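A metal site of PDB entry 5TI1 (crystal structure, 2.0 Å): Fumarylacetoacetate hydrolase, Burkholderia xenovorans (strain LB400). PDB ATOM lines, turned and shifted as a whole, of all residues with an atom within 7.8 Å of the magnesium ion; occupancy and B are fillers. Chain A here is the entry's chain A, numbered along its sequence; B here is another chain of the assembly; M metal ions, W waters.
OE1 of Glu 226 lies within salt-bridge range of NZ of Lys 280 (3.3 Å).
The backbone NH of Glu 226 is in hydrogen-bond range of the side-chain amide oxygen of Asn 259, at 3.1 Å.
The backbone NH (N) of Gly 376 is in hydrogen-bond range of the side-chain carboxylate (OE2) of Glu 228.
N of Tyr 186 sits at hydrogen-bond distance from O of Asp 153 (2.9 Å).
The side-chain hydroxyl (OG) of Ser 262 lies within hydrogen-bond range of the backbone carbonyl oxygen (O) of Asp 260 (2.9 Å).
The side-chain carboxylate (OD2) of Asp 260 lies close to the side-chain hydroxyl (OH) of Tyr 186, 3.1 Å away.
OG1 of Thr 284 lies within hydrogen-bond range of OD1 of Asp 260 (3.5 Å).
OE1 of Glu 226 sits close to OG1 of Thr 377 (3.4 Å).
Merely in contact with the magnesium ion: Tyr 186 (3.7 Å) and Lys 280 (3.4 Å).
The magnesium ion is bound by the side-chain carboxylate of Glu 226 (2.2 Å), the side-chain carboxylate of Asp 153 (2.2 Å), the side-chain carboxylate of Glu 228 (2.3 Å) and the side-chain carboxylate of Asp 260 (2.3 Å).
The magnesium ion has four donor atoms within binding distance.
Slightly farther from the magnesium ion lies water W1 (2.6 Å).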
ATOM      1  N   TYR A 151      25.903 -21.583  21.274  1.00  0.00           N
ATOM      2  CA  TYR A 151      25.168 -20.455  21.814  1.00  0.00           C
ATOM      3  C   TYR A 151      23.703 -20.649  21.485  1.00  0.00           C
ATOM      4  O   TYR A 151      23.328 -20.739  20.313  1.00  0.00           O
ATOM      5  CB  TYR A 151      25.696 -19.113  21.247  1.00  0.00           C
ATOM      6  CG  TYR A 151      24.733 -17.945  21.388  1.00  0.00           C
ATOM      7  CD1 TYR A 151      24.026 -17.726  22.571  1.00  0.00           C
ATOM      8  CD2 TYR A 151      24.551 -17.050  20.343  1.00  0.00           C
ATOM      9  CE1 TYR A 151      23.149 -16.670  22.695  1.00  0.00           C
ATOM     10  CE2 TYR A 151      23.679 -15.967  20.469  1.00  0.00           C
ATOM     11  CZ  TYR A 151      22.984 -15.800  21.645  1.00  0.00           C
ATOM     12  OH  TYR A 151      22.104 -14.746  21.782  1.00  0.00           O
ATOM     13  N   ASP A 153      19.689 -19.262  22.385  1.00  0.00           N
ATOM     14  CA  ASP A 153      18.942 -18.103  22.860  1.00  0.00           C
ATOM     15  C   ASP A 153      17.495 -18.500  23.080  1.00  0.00           C
ATOM     16  O   ASP A 153      16.903 -19.178  22.242  1.00  0.00           O
ATOM     17  CB  ASP A 153      19.049 -16.925  21.883  1.00  0.00           C
ATOM     18  CG  ASP A 153      18.641 -15.611  22.521  1.00  0.00           C
ATOM     19  OD1 ASP A 153      18.825 -15.473  23.748  1.00  0.00           O
ATOM     20  OD2 ASP A 153      18.096 -14.746  21.819  1.00  0.00           O
ATOM     21  N   PHE A 154      16.938 -18.092  24.219  1.00  0.00           N
ATOM     22  CA  PHE A 154      15.589 -18.419  24.621  1.00  0.00           C
ATOM     23  C   PHE A 154      14.694 -17.184  24.463  1.00  0.00           C
ATOM     24  O   PHE A 154      15.067 -16.203  23.809  1.00  0.00           O
ATOM     25  CB  PHE A 154      15.605 -18.970  26.061  1.00  0.00           C
ATOM     26  CG  PHE A 154      16.075 -20.399  26.134  1.00  0.00           C
ATOM     27  CD1 PHE A 154      15.176 -21.433  25.954  1.00  0.00           C
ATOM     28  CD2 PHE A 154      17.416 -20.694  26.316  1.00  0.00           C
ATOM     29  CE1 PHE A 154      15.605 -22.749  25.982  1.00  0.00           C
ATOM     30  CE2 PHE A 154      17.845 -22.016  26.337  1.00  0.00           C
ATOM     31  CZ  PHE A 154      16.942 -23.045  26.178  1.00  0.00           C
ATOM     32  N   TYR A 155      13.520 -17.225  25.080  1.00  0.00           N
ATOM     33  CA  TYR A 155      12.454 -16.279  24.735  1.00  0.00           C
ATOM     34  C   TYR A 155      11.511 -16.144  25.923  1.00  0.00           C
ATOM     35  O   TYR A 155      10.299 -16.037  25.750  1.00  0.00           O
ATOM     36  CB  TYR A 155      11.732 -16.794  23.493  1.00  0.00           C
ATOM     37  CG  TYR A 155      10.881 -15.787  22.745  1.00  0.00           C
ATOM     38  CD1 TYR A 155      11.469 -14.700  22.106  1.00  0.00           C
ATOM     39  CD2 TYR A 155       9.508 -15.957  22.636  1.00  0.00           C
ATOM     40  CE1 TYR A 155      10.696 -13.776  21.406  1.00  0.00           C
ATOM     41  CE2 TYR A 155       8.729 -15.048  21.948  1.00  0.00           C
ATOM     42  CZ  TYR A 155       9.333 -13.959  21.335  1.00  0.00           C
ATOM     43  OH  TYR A 155       8.552 -13.064  20.646  1.00  0.00           O
ATOM     44  N   HIS A 160       7.716  -9.612  27.378  1.00  0.00           N
ATOM     45  CA  HIS A 160       8.284  -9.437  26.039  1.00  0.00           C
ATOM     46  C   HIS A 160       7.442 -10.148  24.979  1.00  0.00           C
ATOM     47  O   HIS A 160       7.001  -9.543  24.004  1.00  0.00           O
ATOM     48  CB  HIS A 160       9.726  -9.959  25.987  1.00  0.00           C
ATOM     49  CG  HIS A 160      10.318  -9.971  24.609  1.00  0.00           C
ATOM     50  ND1 HIS A 160      10.750  -8.829  23.968  1.00  0.00           N
ATOM     51  CD2 HIS A 160      10.549 -10.999  23.747  1.00  0.00           C
ATOM     52  CE1 HIS A 160      11.223  -9.144  22.773  1.00  0.00           C
ATOM     53  NE2 HIS A 160      11.111 -10.456  22.610  1.00  0.00           N
ATOM     54  N   TYR A 186      16.098 -21.144  20.249  1.00  0.00           N
ATOM     55  CA  TYR A 186      16.679 -21.406  18.938  1.00  0.00           C
ATOM     56  C   TYR A 186      18.186 -21.459  19.097  1.00  0.00           C
ATOM     57  O   TYR A 186      18.742 -20.935  20.061  1.00  0.00           O
ATOM     58  CB  TYR A 186      16.255 -20.337  17.915  1.00  0.00           C
ATOM     59  CG  TYR A 186      16.791 -18.945  18.206  1.00  0.00           C
ATOM     60  CD1 TYR A 186      16.189 -18.125  19.155  1.00  0.00           C
ATOM     61  CD2 TYR A 186      17.917 -18.457  17.539  1.00  0.00           C
ATOM     62  CE1 TYR A 186      16.686 -16.854  19.427  1.00  0.00           C
ATOM     63  CE2 TYR A 186      18.424 -17.194  17.805  1.00  0.00           C
ATOM     64  CZ  TYR A 186      17.807 -16.393  18.756  1.00  0.00           C
ATOM     65  OH  TYR A 186      18.323 -15.132  19.024  1.00  0.00           O
ATOM     66  N   ILE A 225      18.401  -3.504  20.247  1.00  0.00           N
ATOM     67  CA  ILE A 225      19.029  -4.313  21.286  1.00  0.00           C
ATOM     68  C   ILE A 225      18.053  -5.416  21.679  1.00  0.00           C
ATOM     69  O   ILE A 225      16.872  -5.377  21.304  1.00  0.00           O
ATOM     70  CB  ILE A 225      19.391  -3.462  22.514  1.00  0.00           C
ATOM     71  CG1 ILE A 225      18.118  -2.937  23.174  1.00  0.00           C
ATOM     72  CG2 ILE A 225      20.303  -2.306  22.124  1.00  0.00           C
ATOM     73  CD1 ILE A 225      18.343  -2.331  24.532  1.00  0.00           C
ATOM     74  N   GLU A 226      18.544  -6.393  22.433  1.00  0.00           N
ATOM     75  CA  GLU A 226      17.690  -7.253  23.245  1.00  0.00           C
ATOM     76  C   GLU A 226      18.406  -7.426  24.579  1.00  0.00           C
ATOM     77  O   GLU A 226      19.468  -8.064  24.641  1.00  0.00           O
ATOM     78  CB  GLU A 226      17.404  -8.599  22.565  1.00  0.00           C
ATOM     79  CG  GLU A 226      16.538  -8.468  21.309  1.00  0.00           C
ATOM     80  CD  GLU A 226      15.802  -9.740  20.894  1.00  0.00           C
ATOM     81  OE1 GLU A 226      14.674  -9.624  20.391  1.00  0.00           O
ATOM     82  OE2 GLU A 226      16.351 -10.862  21.067  1.00  0.00           O
ATOM     83  N   LEU A 227      17.879  -6.809  25.624  1.00  0.00           N
ATOM     84  CA  LEU A 227      18.455  -6.887  26.962  1.00  0.00           C
ATOM     85  C   LEU A 227      18.281  -8.301  27.520  1.00  0.00           C
ATOM     86  O   LEU A 227      17.157  -8.717  27.814  1.00  0.00           O
ATOM     87  CB  LEU A 227      17.802  -5.850  27.857  1.00  0.00           C
ATOM     88  CG  LEU A 227      17.950  -5.936  29.386  1.00  0.00           C
ATOM     89  CD1 LEU A 227      19.403  -6.025  29.807  1.00  0.00           C
ATOM     90  CD2 LEU A 227      17.291  -4.731  30.023  1.00  0.00           C
ATOM     91  N   GLU A 228      19.379  -9.034  27.662  1.00  0.00           N
ATOM     92  CA  GLU A 228      19.322 -10.395  28.156  1.00  0.00           C
ATOM     93  C   GLU A 228      20.427 -10.619  29.192  1.00  0.00           C
ATOM     94  O   GLU A 228      21.289  -9.772  29.422  1.00  0.00           O
ATOM     95  CB  GLU A 228      19.460 -11.412  27.018  1.00  0.00           C
ATOM     96  CG  GLU A 228      18.505 -11.128  25.877  1.00  0.00           C
ATOM     97  CD  GLU A 228      18.491 -12.224  24.836  1.00  0.00           C
ATOM     98  OE1 GLU A 228      18.113 -11.941  23.677  1.00  0.00           O
ATOM     99  OE2 GLU A 228      18.862 -13.366  25.185  1.00  0.00           O
ATOM    100  N   LEU A 258      24.121  -9.882  28.285  1.00  0.00           N
ATOM    101  CA  LEU A 258      24.101 -10.293  26.880  1.00  0.00           C
ATOM    102  C   LEU A 258      23.190  -9.378  26.089  1.00  0.00           C
ATOM    103  O   LEU A 258      21.986  -9.311  26.365  1.00  0.00           O
ATOM    104  CB  LEU A 258      23.631 -11.757  26.745  1.00  0.00           C
ATOM    105  CG  LEU A 258      23.644 -12.420  25.343  1.00  0.00           C
ATOM    106  CD1 LEU A 258      23.783 -13.924  25.486  1.00  0.00           C
ATOM    107  CD2 LEU A 258      22.382 -12.128  24.516  1.00  0.00           C
ATOM    108  N   ASN A 259      23.748  -8.693  25.092  1.00  0.00           N
ATOM    109  CA  ASN A 259      22.960  -7.904  24.152  1.00  0.00           C
ATOM    110  C   ASN A 259      22.872  -8.675  22.835  1.00  0.00           C
ATOM    111  O   ASN A 259      23.857  -8.776  22.103  1.00  0.00           O
ATOM    112  CB  ASN A 259      23.578  -6.529  23.915  1.00  0.00           C
ATOM    113  CG  ASN A 259      22.686  -5.614  23.084  1.00  0.00           C
ATOM    114  OD1 ASN A 259      21.662  -6.050  22.527  1.00  0.00           O
ATOM    115  ND2 ASN A 259      23.079  -4.346  22.974  1.00  0.00           N
ATOM    116  N   ASP A 260      21.690  -9.202  22.539  1.00  0.00           N
ATOM    117  CA  ASP A 260      21.443  -9.917  21.283  1.00  0.00           C
ATOM    118  C   ASP A 260      20.950  -8.913  20.233  1.00  0.00           C
ATOM    119  O   ASP A 260      19.751  -8.764  19.985  1.00  0.00           O
ATOM    120  CB  ASP A 260      20.459 -11.055  21.497  1.00  0.00           C
ATOM    121  CG  ASP A 260      20.178 -11.844  20.235  1.00  0.00           C
ATOM    122  OD1 ASP A 260      21.090 -11.925  19.379  1.00  0.00           O
ATOM    123  OD2 ASP A 260      19.048 -12.354  20.099  1.00  0.00           O
ATOM    124  N   TRP A 261      21.908  -8.187  19.631  1.00  0.00           N
ATOM    125  CA  TRP A 261      21.593  -7.195  18.614  1.00  0.00           C
ATOM    126  C   TRP A 261      20.691  -7.801  17.541  1.00  0.00           C
ATOM    127  O   TRP A 261      20.873  -8.952  17.131  1.00  0.00           O
ATOM    128  CB  TRP A 261      22.854  -6.643  17.954  1.00  0.00           C
ATOM    129  CG  TRP A 261      23.899  -6.134  18.908  1.00  0.00           C
ATOM    130  CD1 TRP A 261      24.970  -6.824  19.404  1.00  0.00           C
ATOM    131  CD2 TRP A 261      24.003  -4.807  19.449  1.00  0.00           C
ATOM    132  NE1 TRP A 261      25.725  -6.020  20.225  1.00  0.00           N
ATOM    133  CE2 TRP A 261      25.151  -4.776  20.273  1.00  0.00           C
ATOM    134  CE3 TRP A 261      23.246  -3.641  19.317  1.00  0.00           C
ATOM    135  CZ2 TRP A 261      25.554  -3.631  20.958  1.00  0.00           C
ATOM    136  CZ3 TRP A 261      23.643  -2.511  20.014  1.00  0.00           C
ATOM    137  CH2 TRP A 261      24.780  -2.511  20.812  1.00  0.00           C
ATOM    138  N   SER A 262      19.710  -7.023  17.094  1.00  0.00           N
ATOM    139  CA  SER A 262      18.649  -7.549  16.245  1.00  0.00           C
ATOM    140  C   SER A 262      18.289  -6.547  15.152  1.00  0.00           C
ATOM    141  O   SER A 262      18.070  -5.373  15.424  1.00  0.00           O
ATOM    142  CB  SER A 262      17.401  -7.911  17.060  1.00  0.00           C
ATOM    143  OG  SER A 262      17.693  -8.942  18.004  1.00  0.00           O
ATOM    144  N   ARG A 264      15.429  -5.897  12.901  1.00  0.00           N
ATOM    145  CA  ARG A 264      14.069  -6.412  12.951  1.00  0.00           C
ATOM    146  C   ARG A 264      13.404  -6.440  11.591  1.00  0.00           C
ATOM    147  O   ARG A 264      12.573  -7.318  11.337  1.00  0.00           O
ATOM    148  CB  ARG A 264      13.259  -5.622  13.965  1.00  0.00           C
ATOM    149  CG  ARG A 264      13.832  -5.808  15.367  1.00  0.00           C
ATOM    150  CD  ARG A 264      12.833  -5.455  16.434  1.00  0.00           C
ATOM    151  NE  ARG A 264      13.434  -5.521  17.764  1.00  0.00           N
ATOM    152  CZ  ARG A 264      13.700  -6.644  18.418  1.00  0.00           C
ATOM    153  NH1 ARG A 264      13.428  -7.826  17.863  1.00  0.00           N
ATOM    154  NH2 ARG A 264      14.251  -6.579  19.622  1.00  0.00           N
ATOM    155  N   GLN A 267      14.729  -9.449   9.996  1.00  0.00           N
ATOM    156  CA  GLN A 267      14.127 -10.632  10.609  1.00  0.00           C
ATOM    157  C   GLN A 267      12.746 -10.921  10.052  1.00  0.00           C
ATOM    158  O   GLN A 267      12.411 -12.080   9.761  1.00  0.00           O
ATOM    159  CB  GLN A 267      14.038 -10.453  12.124  1.00  0.00           C
ATOM    160  CG  GLN A 267      13.437 -11.663  12.852  1.00  0.00           C
ATOM    161  CD  GLN A 267      13.416 -11.466  14.355  1.00  0.00           C
ATOM    162  OE1 GLN A 267      13.855 -12.326  15.113  1.00  0.00           O
ATOM    163  NE2 GLN A 267      12.915 -10.322  14.791  1.00  0.00           N
ATOM    164  N   PRO A 276      14.817 -16.819  13.209  1.00  0.00           N
ATOM    165  CA  PRO A 276      15.717 -15.703  12.931  1.00  0.00           C
ATOM    166  C   PRO A 276      17.073 -16.220  12.517  1.00  0.00           C
ATOM    167  O   PRO A 276      17.559 -17.239  13.018  1.00  0.00           O
ATOM    168  CB  PRO A 276      15.773 -14.928  14.256  1.00  0.00           C
ATOM    169  CG  PRO A 276      15.404 -15.925  15.302  1.00  0.00           C
ATOM    170  CD  PRO A 276      14.430 -16.890  14.628  1.00  0.00           C
ATOM    171  N   LYS A 280      20.144 -11.836  13.419  1.00  0.00           N
ATOM    172  CA  LYS A 280      20.712 -12.026  14.746  1.00  0.00           C
ATOM    173  C   LYS A 280      22.200 -12.323  14.729  1.00  0.00           C
ATOM    174  O   LYS A 280      22.888 -11.979  15.696  1.00  0.00           O
ATOM    175  CB  LYS A 280      20.017 -13.192  15.470  1.00  0.00           C
ATOM    176  CG  LYS A 280      18.522 -13.054  15.618  1.00  0.00           C
ATOM    177  CD  LYS A 280      18.157 -12.055  16.680  1.00  0.00           C
ATOM    178  CE  LYS A 280      16.824 -12.412  17.316  1.00  0.00           C
ATOM    179  NZ  LYS A 280      16.611 -11.624  18.550  1.00  0.00           N
ATOM    180  N   THR A 284      26.544 -10.466  18.678  1.00  0.00           N
ATOM    181  CA  THR A 284      25.961 -10.630  20.007  1.00  0.00           C
ATOM    182  C   THR A 284      27.047 -10.241  20.998  1.00  0.00           C
ATOM    183  O   THR A 284      28.160 -10.758  20.935  1.00  0.00           O
ATOM    184  CB  THR A 284      25.496 -12.074  20.246  1.00  0.00           C
ATOM    185  OG1 THR A 284      24.521 -12.425  19.256  1.00  0.00           O
ATOM    186  CG2 THR A 284      24.854 -12.220  21.621  1.00  0.00           C
ATOM    187  N   GLY A 374      21.340 -17.662  26.324  1.00  0.00           N
ATOM    188  CA  GLY A 374      20.701 -16.366  26.522  1.00  0.00           C
ATOM    189  C   GLY A 374      19.262 -16.522  27.010  1.00  0.00           C
ATOM    190  O   GLY A 374      18.528 -17.418  26.580  1.00  0.00           O
ATOM    191  N   SER A 375      18.857 -15.612  27.895  1.00  0.00           N
ATOM    192  CA  SER A 375      17.556 -15.723  28.551  1.00  0.00           C
ATOM    193  C   SER A 375      16.397 -15.394  27.620  1.00  0.00           C
ATOM    194  O   SER A 375      15.259 -15.779  27.914  1.00  0.00           O
ATOM    195  CB  SER A 375      17.483 -14.783  29.756  1.00  0.00           C
ATOM    196  OG  SER A 375      17.677 -13.445  29.329  1.00  0.00           O
ATOM    197  N   GLY A 376      16.666 -14.679  26.544  1.00  0.00           N
ATOM    198  CA  GLY A 376      15.653 -13.918  25.848  1.00  0.00           C
ATOM    199  C   GLY A 376      15.518 -12.522  26.447  1.00  0.00           C
ATOM    200  O   GLY A 376      15.971 -12.256  27.557  1.00  0.00           O
ATOM    201  N   THR A 377      14.915 -11.623  25.661  1.00  0.00           N
ATOM    202  CA  THR A 377      14.726 -10.233  26.080  1.00  0.00           C
ATOM    203  C   THR A 377      13.998 -10.172  27.408  1.00  0.00           C
ATOM    204  O   THR A 377      12.959 -10.820  27.588  1.00  0.00           O
ATOM    205  CB  THR A 377      13.927  -9.466  25.027  1.00  0.00           C
ATOM    206  OG1 THR A 377      14.581  -9.579  23.752  1.00  0.00           O
ATOM    207  CG2 THR A 377      13.817  -7.983  25.399  1.00  0.00           C
ATOM    208  N   LEU B 274      10.378 -19.415  16.406  1.00  0.00           N
ATOM    209  CA  LEU B 274      11.837 -19.337  16.375  1.00  0.00           C
ATOM    210  C   LEU B 274      12.494 -20.501  15.639  1.00  0.00           C
ATOM    211  O   LEU B 274      13.719 -20.582  15.635  1.00  0.00           O
ATOM    212  CB  LEU B 274      12.382 -19.261  17.805  1.00  0.00           C
ATOM    213  CG  LEU B 274      11.891 -18.080  18.654  1.00  0.00           C
ATOM    214  CD1 LEU B 274      12.350 -18.221  20.091  1.00  0.00           C
ATOM    215  CD2 LEU B 274      12.323 -16.726  18.058  1.00  0.00           C
HETATM  216 MG    MG M   1      17.384 -12.662  21.667  1.00  0.00          MG
HETATM  217  O   HOH W   1      15.076 -13.928  21.961  1.00  0.00           O
